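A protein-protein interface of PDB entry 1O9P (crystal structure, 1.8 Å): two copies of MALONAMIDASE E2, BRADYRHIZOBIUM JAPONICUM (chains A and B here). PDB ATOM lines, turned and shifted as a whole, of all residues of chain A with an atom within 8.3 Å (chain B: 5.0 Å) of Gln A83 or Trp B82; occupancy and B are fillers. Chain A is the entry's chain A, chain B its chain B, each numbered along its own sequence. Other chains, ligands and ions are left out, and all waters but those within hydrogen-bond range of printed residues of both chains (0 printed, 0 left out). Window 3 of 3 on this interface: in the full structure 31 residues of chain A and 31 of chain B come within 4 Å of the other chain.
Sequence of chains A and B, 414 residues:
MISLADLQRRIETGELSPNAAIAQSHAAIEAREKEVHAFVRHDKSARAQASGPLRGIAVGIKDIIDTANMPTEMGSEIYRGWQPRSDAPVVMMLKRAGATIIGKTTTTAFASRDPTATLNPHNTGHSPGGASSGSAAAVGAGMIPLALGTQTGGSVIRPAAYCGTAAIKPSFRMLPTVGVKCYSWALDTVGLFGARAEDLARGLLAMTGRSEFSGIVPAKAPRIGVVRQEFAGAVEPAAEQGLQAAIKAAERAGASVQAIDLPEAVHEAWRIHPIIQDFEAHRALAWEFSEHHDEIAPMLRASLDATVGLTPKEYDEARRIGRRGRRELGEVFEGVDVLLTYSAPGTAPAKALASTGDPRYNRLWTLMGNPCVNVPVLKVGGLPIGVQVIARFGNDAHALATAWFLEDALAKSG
Among the printed residues, merely in contact across the chains: Arg A85 with Trp B82, Trp A82 with Gln B83, Gln A83 with Trp B82, Arg A85 with Tyr B79, Trp A82 with Trp B82, Pro A84 with Trp B82 and Trp A82 with Pro B84.
Trp A82 touches its own counterpart, Trp B82.
Trp A82 touches Gln B83, and with the chains exchanged Gln A83 touches Trp B82.
Trp A82 touches Pro B84, and with the chains exchanged Pro A84 touches Trp B82.
10 positions are printed for both chains.
Of the 8 pairs that touch across the chains among the printed residues, 5 have their exchanged pair printed and touching as well.
Gln A83 touches one residue of chain B.
Of chain A, only Trp A82 (3.6 Å), Gln A83 (3.4 Å), Pro A84 (3.9 Å) and Arg A85 (3.3 Å) come within 4 Å of Trp B82.
Gly B81 touches none of the printed residues of chain A.
Printed residues of chain B within 4 Å of Ser A86: Tyr B79.
Of the printed residues of chain B, Trp A82 touches Trp B82, Gln B83 and Pro B84.
The nearest printed residue of chain B that does not touch Gln A83 is Gln B83 (6.7 Å).
The nearest residue of chain A that does not touch Trp B82 is Ser A86 (5.8 Å).
The side-chain hydroxyl (OG) of Ser A86 sits at hydrogen-bond distance from the side-chain hydroxyl (OH) of Tyr B79 (3.5 Å).
O of Trp A82 lies within hydrogen-bond range of N of Thr A72, at 3.0 Å.
The backbone carbonyl oxygen (O) of Thr A67 sits close to the side-chain amide oxygen (OE1) of Gln A83, 2.9 Å away.
The side-chain amide oxygen (OE1) of Gln A83 lies close to the backbone carbonyl oxygen (O) of Met A70 (3.0 Å).
O of Ala A68 sits close to OE1 of Gln A83 (3.2 Å).
N of Thr B72 lies within hydrogen-bond range of O of Trp B82.
Of the 10 printed residues of chain B, 4 touch a printed residue of chain A.
Hydrophobic or aromatic side chains of chain B that line the printed part of chain A: Tyr B79 and Trp B82.
Of the 20 printed residues of chain A, 5 touch a printed residue of chain B.
Among the printed residues, 8 pairs touch across the chains.
Among the printed residues, no Asp or Glu carboxylate lies within 4 Å of a Lys or Arg side-chain nitrogen of the other chain.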
ATOM      1  N   ARG A  41      11.109  29.269 -20.436  1.00  0.00           N
ATOM      2  CA  ARG A  41      11.894  28.161 -20.944  1.00  0.00           C
ATOM      3  C   ARG A  41      12.203  28.354 -22.421  1.00  0.00           C
ATOM      4  O   ARG A  41      11.350  28.765 -23.219  1.00  0.00           O
ATOM      5  CB  ARG A  41      11.172  26.831 -20.715  1.00  0.00           C
ATOM      6  CG  ARG A  41       9.852  26.697 -21.426  1.00  0.00           C
ATOM      7  CD  ARG A  41       9.083  25.489 -20.915  1.00  0.00           C
ATOM      8  NE  ARG A  41       8.828  25.563 -19.476  1.00  0.00           N
ATOM      9  CZ  ARG A  41       9.600  25.012 -18.543  1.00  0.00           C
ATOM     10  NH1 ARG A  41      10.688  24.335 -18.890  1.00  0.00           N
ATOM     11  NH2 ARG A  41       9.281  25.138 -17.262  1.00  0.00           N
ATOM     12  N   ASP A  66      -1.306  27.076 -24.067  1.00  0.00           N
ATOM     13  CA  ASP A  66      -0.919  25.662 -24.088  1.00  0.00           C
ATOM     14  C   ASP A  66       0.050  25.209 -25.170  1.00  0.00           C
ATOM     15  O   ASP A  66      -0.118  25.533 -26.346  1.00  0.00           O
ATOM     16  CB  ASP A  66      -2.151  24.756 -24.223  1.00  0.00           C
ATOM     17  CG  ASP A  66      -3.002  24.712 -22.975  1.00  0.00           C
ATOM     18  OD1 ASP A  66      -2.533  25.139 -21.902  1.00  0.00           O
ATOM     19  OD2 ASP A  66      -4.149  24.227 -23.078  1.00  0.00           O
ATOM     20  N   THR A  67       1.049  24.433 -24.754  1.00  0.00           N
ATOM     21  CA  THR A  67       2.015  23.823 -25.663  1.00  0.00           C
ATOM     22  C   THR A  67       2.116  22.375 -25.192  1.00  0.00           C
ATOM     23  O   THR A  67       2.122  22.106 -23.987  1.00  0.00           O
ATOM     24  CB  THR A  67       3.414  24.503 -25.623  1.00  0.00           C
ATOM     25  OG1 THR A  67       3.810  24.745 -24.270  1.00  0.00           O
ATOM     26  CG2 THR A  67       3.381  25.818 -26.402  1.00  0.00           C
ATOM     27  N   ALA A  68       2.169  21.442 -26.135  1.00  0.00           N
ATOM     28  CA  ALA A  68       2.228  20.022 -25.793  1.00  0.00           C
ATOM     29  C   ALA A  68       3.621  19.477 -25.490  1.00  0.00           C
ATOM     30  O   ALA A  68       3.752  18.452 -24.828  1.00  0.00           O
ATOM     31  CB  ALA A  68       1.594  19.200 -26.920  1.00  0.00           C
ATOM     32  N   ASN A  69       4.654  20.163 -25.967  1.00  0.00           N
ATOM     33  CA  ASN A  69       6.030  19.705 -25.775  1.00  0.00           C
ATOM     34  C   ASN A  69       6.816  20.476 -24.714  1.00  0.00           C
ATOM     35  O   ASN A  69       7.966  20.138 -24.415  1.00  0.00           O
ATOM     36  CB  ASN A  69       6.766  19.787 -27.107  1.00  0.00           C
ATOM     37  CG  ASN A  69       6.957  21.214 -27.572  1.00  0.00           C
ATOM     38  OD1 ASN A  69       6.092  22.067 -27.364  1.00  0.00           O
ATOM     39  ND2 ASN A  69       8.088  21.483 -28.217  1.00  0.00           N
ATOM     40  N   MET A  70       6.196  21.512 -24.161  1.00  0.00           N
ATOM     41  CA  MET A  70       6.812  22.347 -23.130  1.00  0.00           C
ATOM     42  C   MET A  70       5.758  22.668 -22.093  1.00  0.00           C
ATOM     43  O   MET A  70       4.586  22.820 -22.425  1.00  0.00           O
ATOM     44  CB  MET A  70       7.284  23.681 -23.702  1.00  0.00           C
ATOM     45  CG  MET A  70       8.520  23.655 -24.537  1.00  0.00           C
ATOM     46  SD  MET A  70       8.789  25.332 -25.127  1.00  0.00           S
ATOM     47  CE  MET A  70       8.374  25.147 -26.846  1.00  0.00           C
ATOM     48  N   PRO A  71       6.163  22.797 -20.822  1.00  0.00           N
ATOM     49  CA  PRO A  71       5.168  23.116 -19.797  1.00  0.00           C
ATOM     50  C   PRO A  71       4.498  24.468 -20.068  1.00  0.00           C
ATOM     51  O   PRO A  71       4.996  25.283 -20.847  1.00  0.00           O
ATOM     52  CB  PRO A  71       5.993  23.139 -18.510  1.00  0.00           C
ATOM     53  CG  PRO A  71       7.069  22.119 -18.781  1.00  0.00           C
ATOM     54  CD  PRO A  71       7.461  22.449 -20.213  1.00  0.00           C
ATOM     55  N   THR A  72       3.353  24.682 -19.430  1.00  0.00           N
ATOM     56  CA  THR A  72       2.606  25.932 -19.537  1.00  0.00           C
ATOM     57  C   THR A  72       2.265  26.198 -18.076  1.00  0.00           C
ATOM     58  O   THR A  72       1.281  25.677 -17.545  1.00  0.00           O
ATOM     59  CB  THR A  72       1.341  25.748 -20.387  1.00  0.00           C
ATOM     60  OG1 THR A  72       1.715  25.248 -21.681  1.00  0.00           O
ATOM     61  CG2 THR A  72       0.618  27.077 -20.567  1.00  0.00           C
ATOM     62  N   GLU A  73       3.110  26.998 -17.429  1.00  0.00           N
ATOM     63  CA  GLU A  73       2.985  27.273 -16.002  1.00  0.00           C
ATOM     64  C   GLU A  73       2.170  28.475 -15.524  1.00  0.00           C
ATOM     65  O   GLU A  73       2.126  28.753 -14.328  1.00  0.00           O
ATOM     66  CB  GLU A  73       4.399  27.298 -15.405  1.00  0.00           C
ATOM     67  CG  GLU A  73       5.187  26.043 -15.783  1.00  0.00           C
ATOM     68  CD  GLU A  73       6.582  25.999 -15.192  1.00  0.00           C
ATOM     69  OE1 GLU A  73       7.348  26.958 -15.411  1.00  0.00           O
ATOM     70  OE2 GLU A  73       6.911  24.994 -14.519  1.00  0.00           O
ATOM     71  N   MET A  74       1.528  29.174 -16.454  1.00  0.00           N
ATOM     72  CA  MET A  74       0.666  30.313 -16.136  1.00  0.00           C
ATOM     73  C   MET A  74       1.288  31.411 -15.275  1.00  0.00           C
ATOM     74  O   MET A  74       0.562  32.212 -14.685  1.00  0.00           O
ATOM     75  CB  MET A  74      -0.599  29.818 -15.425  1.00  0.00           C
ATOM     76  CG  MET A  74      -1.162  28.504 -15.948  1.00  0.00           C
ATOM     77  SD  MET A  74      -1.620  28.571 -17.689  1.00  0.00           S
ATOM     78  CE  MET A  74      -2.296  26.896 -17.932  1.00  0.00           C
ATOM     79  N   TYR A  79       0.801  26.162 -11.025  1.00  0.00           N
ATOM     80  CA  TYR A  79       0.935  25.362 -12.236  1.00  0.00           C
ATOM     81  C   TYR A  79       2.375  25.008 -12.563  1.00  0.00           C
ATOM     82  O   TYR A  79       2.727  24.789 -13.724  1.00  0.00           O
ATOM     83  CB  TYR A  79       0.295  26.084 -13.427  1.00  0.00           C
ATOM     84  CG  TYR A  79      -1.217  26.074 -13.389  1.00  0.00           C
ATOM     85  CD1 TYR A  79      -1.925  26.960 -12.576  1.00  0.00           C
ATOM     86  CD2 TYR A  79      -1.941  25.156 -14.148  1.00  0.00           C
ATOM     87  CE1 TYR A  79      -3.320  26.930 -12.524  1.00  0.00           C
ATOM     88  CE2 TYR A  79      -3.331  25.116 -14.104  1.00  0.00           C
ATOM     89  CZ  TYR A  79      -4.015  26.007 -13.289  1.00  0.00           C
ATOM     90  OH  TYR A  79      -5.393  25.971 -13.252  1.00  0.00           O
ATOM     91  N   ARG A  80       3.218  24.952 -11.539  1.00  0.00           N
ATOM     92  CA  ARG A  80       4.613  24.595 -11.756  1.00  0.00           C
ATOM     93  C   ARG A  80       4.681  23.198 -12.371  1.00  0.00           C
ATOM     94  O   ARG A  80       4.051  22.260 -11.878  1.00  0.00           O
ATOM     95  CB  ARG A  80       5.380  24.614 -10.434  1.00  0.00           C
ATOM     96  CG  ARG A  80       6.829  24.184 -10.567  1.00  0.00           C
ATOM     97  CD  ARG A  80       7.502  24.094  -9.211  1.00  0.00           C
ATOM     98  NE  ARG A  80       8.856  23.564  -9.317  1.00  0.00           N
ATOM     99  CZ  ARG A  80       9.665  23.366  -8.281  1.00  0.00           C
ATOM    100  NH1 ARG A  80       9.256  23.655  -7.050  1.00  0.00           N
ATOM    101  NH2 ARG A  80      10.884  22.881  -8.477  1.00  0.00           N
ATOM    102  N   GLY A  81       5.430  23.073 -13.461  1.00  0.00           N
ATOM    103  CA  GLY A  81       5.574  21.793 -14.132  1.00  0.00           C
ATOM    104  C   GLY A  81       4.349  21.302 -14.889  1.00  0.00           C
ATOM    105  O   GLY A  81       4.388  20.232 -15.498  1.00  0.00           O
ATOM    106  N   TRP A  82       3.262  22.069 -14.857  1.00  0.00           N
ATOM    107  CA  TRP A  82       2.037  21.666 -15.551  1.00  0.00           C
ATOM    108  C   TRP A  82       2.310  21.441 -17.032  1.00  0.00           C
ATOM    109  O   TRP A  82       2.880  22.301 -17.700  1.00  0.00           O
ATOM    110  CB  TRP A  82       0.945  22.728 -15.390  1.00  0.00           C
ATOM    111  CG  TRP A  82      -0.269  22.429 -16.229  1.00  0.00           C
ATOM    112  CD1 TRP A  82      -0.754  23.177 -17.260  1.00  0.00           C
ATOM    113  CD2 TRP A  82      -1.109  21.272 -16.142  1.00  0.00           C
ATOM    114  NE1 TRP A  82      -1.845  22.559 -17.825  1.00  0.00           N
ATOM    115  CE2 TRP A  82      -2.085  21.386 -17.159  1.00  0.00           C
ATOM    116  CE3 TRP A  82      -1.132  20.146 -15.305  1.00  0.00           C
ATOM    117  CZ2 TRP A  82      -3.077  20.416 -17.363  1.00  0.00           C
ATOM    118  CZ3 TRP A  82      -2.121  19.178 -15.509  1.00  0.00           C
ATOM    119  CH2 TRP A  82      -3.079  19.324 -16.533  1.00  0.00           C
ATOM    120  N   GLN A  83       1.890  20.287 -17.547  1.00  0.00           N
ATOM    121  CA  GLN A  83       2.122  19.965 -18.949  1.00  0.00           C
ATOM    122  C   GLN A  83       0.857  19.641 -19.731  1.00  0.00           C
ATOM    123  O   GLN A  83       0.306  18.545 -19.609  1.00  0.00           O
ATOM    124  CB  GLN A  83       3.078  18.776 -19.062  1.00  0.00           C
ATOM    125  CG  GLN A  83       3.392  18.374 -20.504  1.00  0.00           C
ATOM    126  CD  GLN A  83       3.961  19.528 -21.311  1.00  0.00           C
ATOM    127  OE1 GLN A  83       3.280  20.117 -22.157  1.00  0.00           O
ATOM    128  NE2 GLN A  83       5.212  19.871 -21.039  1.00  0.00           N
ATOM    129  N   PRO A  84       0.388  20.587 -20.555  1.00  0.00           N
ATOM    130  CA  PRO A  84      -0.819  20.341 -21.345  1.00  0.00           C
ATOM    131  C   PRO A  84      -0.593  19.171 -22.295  1.00  0.00           C
ATOM    132  O   PRO A  84       0.533  18.909 -22.729  1.00  0.00           O
ATOM    133  CB  PRO A  84      -1.008  21.651 -22.104  1.00  0.00           C
ATOM    134  CG  PRO A  84      -0.421  22.672 -21.177  1.00  0.00           C
ATOM    135  CD  PRO A  84       0.835  21.983 -20.705  1.00  0.00           C
ATOM    136  N   ARG A  85      -1.674  18.477 -22.617  1.00  0.00           N
ATOM    137  CA  ARG A  85      -1.625  17.342 -23.522  1.00  0.00           C
ATOM    138  C   ARG A  85      -1.528  17.822 -24.972  1.00  0.00           C
ATOM    139  O   ARG A  85      -0.864  17.198 -25.801  1.00  0.00           O
ATOM    140  CB  ARG A  85      -2.889  16.497 -23.319  1.00  0.00           C
ATOM    141  CG  ARG A  85      -3.160  15.421 -24.365  1.00  0.00           C
ATOM    142  CD  ARG A  85      -2.038  14.407 -24.481  1.00  0.00           C
ATOM    143  NE  ARG A  85      -2.455  13.257 -25.285  1.00  0.00           N
ATOM    144  CZ  ARG A  85      -1.626  12.474 -25.971  1.00  0.00           C
ATOM    145  NH1 ARG A  85      -0.319  12.711 -25.959  1.00  0.00           N
ATOM    146  NH2 ARG A  85      -2.108  11.455 -26.677  1.00  0.00           N
ATOM    147  N   SER A  86      -2.164  18.955 -25.261  1.00  0.00           N
ATOM    148  CA  SER A  86      -2.193  19.490 -26.618  1.00  0.00           C
ATOM    149  C   SER A  86      -1.696  20.922 -26.779  1.00  0.00           C
ATOM    150  O   SER A  86      -1.571  21.668 -25.807  1.00  0.00           O
ATOM    151  CB  SER A  86      -3.624  19.423 -27.147  1.00  0.00           C
ATOM    152  OG  SER A  86      -4.480  20.248 -26.370  1.00  0.00           O
ATOM    153  N   ASP A  87      -1.407  21.289 -28.024  1.00  0.00           N
ATOM    154  CA  ASP A  87      -0.977  22.641 -28.358  1.00  0.00           C
ATOM    155  C   ASP A  87      -2.261  23.421 -28.569  1.00  0.00           C
ATOM    156  O   ASP A  87      -3.210  22.904 -29.161  1.00  0.00           O
ATOM    157  CB  ASP A  87      -0.193  22.682 -29.674  1.00  0.00           C
ATOM    158  CG  ASP A  87       1.199  22.113 -29.552  1.00  0.00           C
ATOM    159  OD1 ASP A  87       1.952  22.561 -28.664  1.00  0.00           O
ATOM    160  OD2 ASP A  87       1.543  21.226 -30.360  1.00  0.00           O
ATOM    161  N   LYS A 104       8.652  29.429 -24.256  1.00  0.00           N
ATOM    162  CA  LYS A 104       7.520  30.059 -23.588  1.00  0.00           C
ATOM    163  C   LYS A 104       8.048  31.336 -22.952  1.00  0.00           C
ATOM    164  O   LYS A 104       9.036  31.309 -22.215  1.00  0.00           O
ATOM    165  CB  LYS A 104       6.937  29.145 -22.502  1.00  0.00           C
ATOM    166  CG  LYS A 104       6.589  27.731 -22.969  1.00  0.00           C
ATOM    167  CD  LYS A 104       5.681  27.717 -24.208  1.00  0.00           C
ATOM    168  CE  LYS A 104       4.275  28.224 -23.903  1.00  0.00           C
ATOM    169  NZ  LYS A 104       3.519  27.273 -23.025  1.00  0.00           N
ATOM    170  N   PRO B  71     -10.325  11.931 -13.994  1.00  0.00           N
ATOM    171  CA  PRO B  71      -9.860  12.174 -15.362  1.00  0.00           C
ATOM    172  C   PRO B  71     -10.947  12.799 -16.247  1.00  0.00           C
ATOM    173  O   PRO B  71     -12.134  12.719 -15.949  1.00  0.00           O
ATOM    174  CB  PRO B  71      -9.474  10.777 -15.855  1.00  0.00           C
ATOM    175  CG  PRO B  71      -9.151  10.030 -14.596  1.00  0.00           C
ATOM    176  CD  PRO B  71     -10.222  10.503 -13.650  1.00  0.00           C
ATOM    177  N   THR B  72     -10.522  13.436 -17.326  1.00  0.00           N
ATOM    178  CA  THR B  72     -11.443  14.031 -18.289  1.00  0.00           C
ATOM    179  C   THR B  72     -10.884  13.498 -19.604  1.00  0.00           C
ATOM    180  O   THR B  72      -9.934  14.054 -20.160  1.00  0.00           O
ATOM    181  CB  THR B  72     -11.390  15.566 -18.235  1.00  0.00           C
ATOM    182  OG1 THR B  72     -11.731  16.004 -16.910  1.00  0.00           O
ATOM    183  CG2 THR B  72     -12.373  16.166 -19.229  1.00  0.00           C
ATOM    184  N   GLU B  73     -11.472  12.401 -20.084  1.00  0.00           N
ATOM    185  CA  GLU B  73     -10.988  11.722 -21.283  1.00  0.00           C
ATOM    186  C   GLU B  73     -11.588  12.056 -22.651  1.00  0.00           C
ATOM    187  O   GLU B  73     -11.230  11.430 -23.647  1.00  0.00           O
ATOM    188  CB  GLU B  73     -11.030  10.208 -21.034  1.00  0.00           C
ATOM    189  CG  GLU B  73     -10.279   9.815 -19.750  1.00  0.00           C
ATOM    190  CD  GLU B  73     -10.292   8.320 -19.471  1.00  0.00           C
ATOM    191  OE1 GLU B  73     -11.386   7.717 -19.474  1.00  0.00           O
ATOM    192  OE2 GLU B  73      -9.204   7.751 -19.237  1.00  0.00           O
ATOM    193  N   MET B  74     -12.490  13.034 -22.700  1.00  0.00           N
ATOM    194  CA  MET B  74     -13.081  13.487 -23.961  1.00  0.00           C
ATOM    195  C   MET B  74     -13.741  12.399 -24.807  1.00  0.00           C
ATOM    196  O   MET B  74     -14.018  12.618 -25.991  1.00  0.00           O
ATOM    197  CB  MET B  74     -12.001  14.161 -24.816  1.00  0.00           C
ATOM    198  CG  MET B  74     -11.008  15.014 -24.034  1.00  0.00           C
ATOM    199  SD  MET B  74     -11.799  16.330 -23.098  1.00  0.00           S
ATOM    200  CE  MET B  74     -10.388  16.965 -22.141  1.00  0.00           C
ATOM    201  N   TYR B  79      -7.141  10.970 -25.285  1.00  0.00           N
ATOM    202  CA  TYR B  79      -7.037  11.529 -23.942  1.00  0.00           C
ATOM    203  C   TYR B  79      -7.217  10.493 -22.833  1.00  0.00           C
ATOM    204  O   TYR B  79      -7.631  10.822 -21.719  1.00  0.00           O
ATOM    205  CB  TYR B  79      -8.041  12.675 -23.764  1.00  0.00           C
ATOM    206  CG  TYR B  79      -7.652  13.929 -24.517  1.00  0.00           C
ATOM    207  CD1 TYR B  79      -7.864  14.041 -25.893  1.00  0.00           C
ATOM    208  CD2 TYR B  79      -7.037  14.990 -23.858  1.00  0.00           C
ATOM    209  CE1 TYR B  79      -7.467  15.185 -26.592  1.00  0.00           C
ATOM    210  CE2 TYR B  79      -6.636  16.129 -24.540  1.00  0.00           C
ATOM    211  CZ  TYR B  79      -6.854  16.225 -25.907  1.00  0.00           C
ATOM    212  OH  TYR B  79      -6.460  17.369 -26.566  1.00  0.00           O
ATOM    213  N   ARG B  80      -6.903   9.237 -23.133  1.00  0.00           N
ATOM    214  CA  ARG B  80      -7.020   8.185 -22.130  1.00  0.00           C
ATOM    215  C   ARG B  80      -6.119   8.553 -20.955  1.00  0.00           C
ATOM    216  O   ARG B  80      -4.940   8.833 -21.143  1.00  0.00           O
ATOM    217  CB  ARG B  80      -6.567   6.845 -22.709  1.00  0.00           C
ATOM    218  CG  ARG B  80      -6.729   5.666 -21.760  1.00  0.00           C
ATOM    219  CD  ARG B  80      -8.181   5.226 -21.667  1.00  0.00           C
ATOM    220  NE  ARG B  80      -8.340   4.050 -20.814  1.00  0.00           N
ATOM    221  CZ  ARG B  80      -8.215   4.061 -19.490  1.00  0.00           C
ATOM    222  NH1 ARG B  80      -7.931   5.191 -18.854  1.00  0.00           N
ATOM    223  NH2 ARG B  80      -8.367   2.939 -18.800  1.00  0.00           N
ATOM    224  N   GLY B  81      -6.684   8.561 -19.751  1.00  0.00           N
ATOM    225  CA  GLY B  81      -5.913   8.890 -18.565  1.00  0.00           C
ATOM    226  C   GLY B  81      -5.584  10.366 -18.375  1.00  0.00           C
ATOM    227  O   GLY B  81      -4.867  10.717 -17.442  1.00  0.00           O
ATOM    228  N   TRP B  82      -6.094  11.235 -19.242  1.00  0.00           N
ATOM    229  CA  TRP B  82      -5.807  12.663 -19.116  1.00  0.00           C
ATOM    230  C   TRP B  82      -6.413  13.253 -17.848  1.00  0.00           C
ATOM    231  O   TRP B  82      -7.598  13.074 -17.581  1.00  0.00           O
ATOM    232  CB  TRP B  82      -6.326  13.429 -20.334  1.00  0.00           C
ATOM    233  CG  TRP B  82      -6.176  14.914 -20.178  1.00  0.00           C
ATOM    234  CD1 TRP B  82      -7.180  15.833 -20.090  1.00  0.00           C
ATOM    235  CD2 TRP B  82      -4.951  15.643 -20.034  1.00  0.00           C
ATOM    236  NE1 TRP B  82      -6.659  17.090 -19.899  1.00  0.00           N
ATOM    237  CE2 TRP B  82      -5.291  17.003 -19.859  1.00  0.00           C
ATOM    238  CE3 TRP B  82      -3.594  15.278 -20.030  1.00  0.00           C
ATOM    239  CZ2 TRP B  82      -4.327  18.005 -19.683  1.00  0.00           C
ATOM    240  CZ3 TRP B  82      -2.631  16.277 -19.853  1.00  0.00           C
ATOM    241  CH2 TRP B  82      -3.006  17.623 -19.682  1.00  0.00           C
ATOM    242  N   GLN B  83      -5.595  13.966 -17.076  1.00  0.00           N
ATOM    243  CA  GLN B  83      -6.047  14.566 -15.828  1.00  0.00           C
ATOM    244  C   GLN B  83      -5.844  16.075 -15.760  1.00  0.00           C
ATOM    245  O   GLN B  83      -4.720  16.549 -15.580  1.00  0.00           O
ATOM    246  CB  GLN B  83      -5.323  13.917 -14.641  1.00  0.00           C
ATOM    247  CG  GLN B  83      -5.733  14.471 -13.280  1.00  0.00           C
ATOM    248  CD  GLN B  83      -7.236  14.426 -13.067  1.00  0.00           C
ATOM    249  OE1 GLN B  83      -7.912  15.460 -13.068  1.00  0.00           O
ATOM    250  NE2 GLN B  83      -7.766  13.226 -12.889  1.00  0.00           N
ATOM    251  N   PRO B  84      -6.931  16.850 -15.920  1.00  0.00           N
ATOM    252  CA  PRO B  84      -6.833  18.312 -15.861  1.00  0.00           C
ATOM    253  C   PRO B  84      -6.343  18.743 -14.486  1.00  0.00           C
ATOM    254  O   PRO B  84      -6.537  18.031 -13.499  1.00  0.00           O
ATOM    255  CB  PRO B  84      -8.268  18.766 -16.115  1.00  0.00           C
ATOM    256  CG  PRO B  84      -8.796  17.705 -17.031  1.00  0.00           C
ATOM    257  CD  PRO B  84      -8.266  16.434 -16.389  1.00  0.00           C
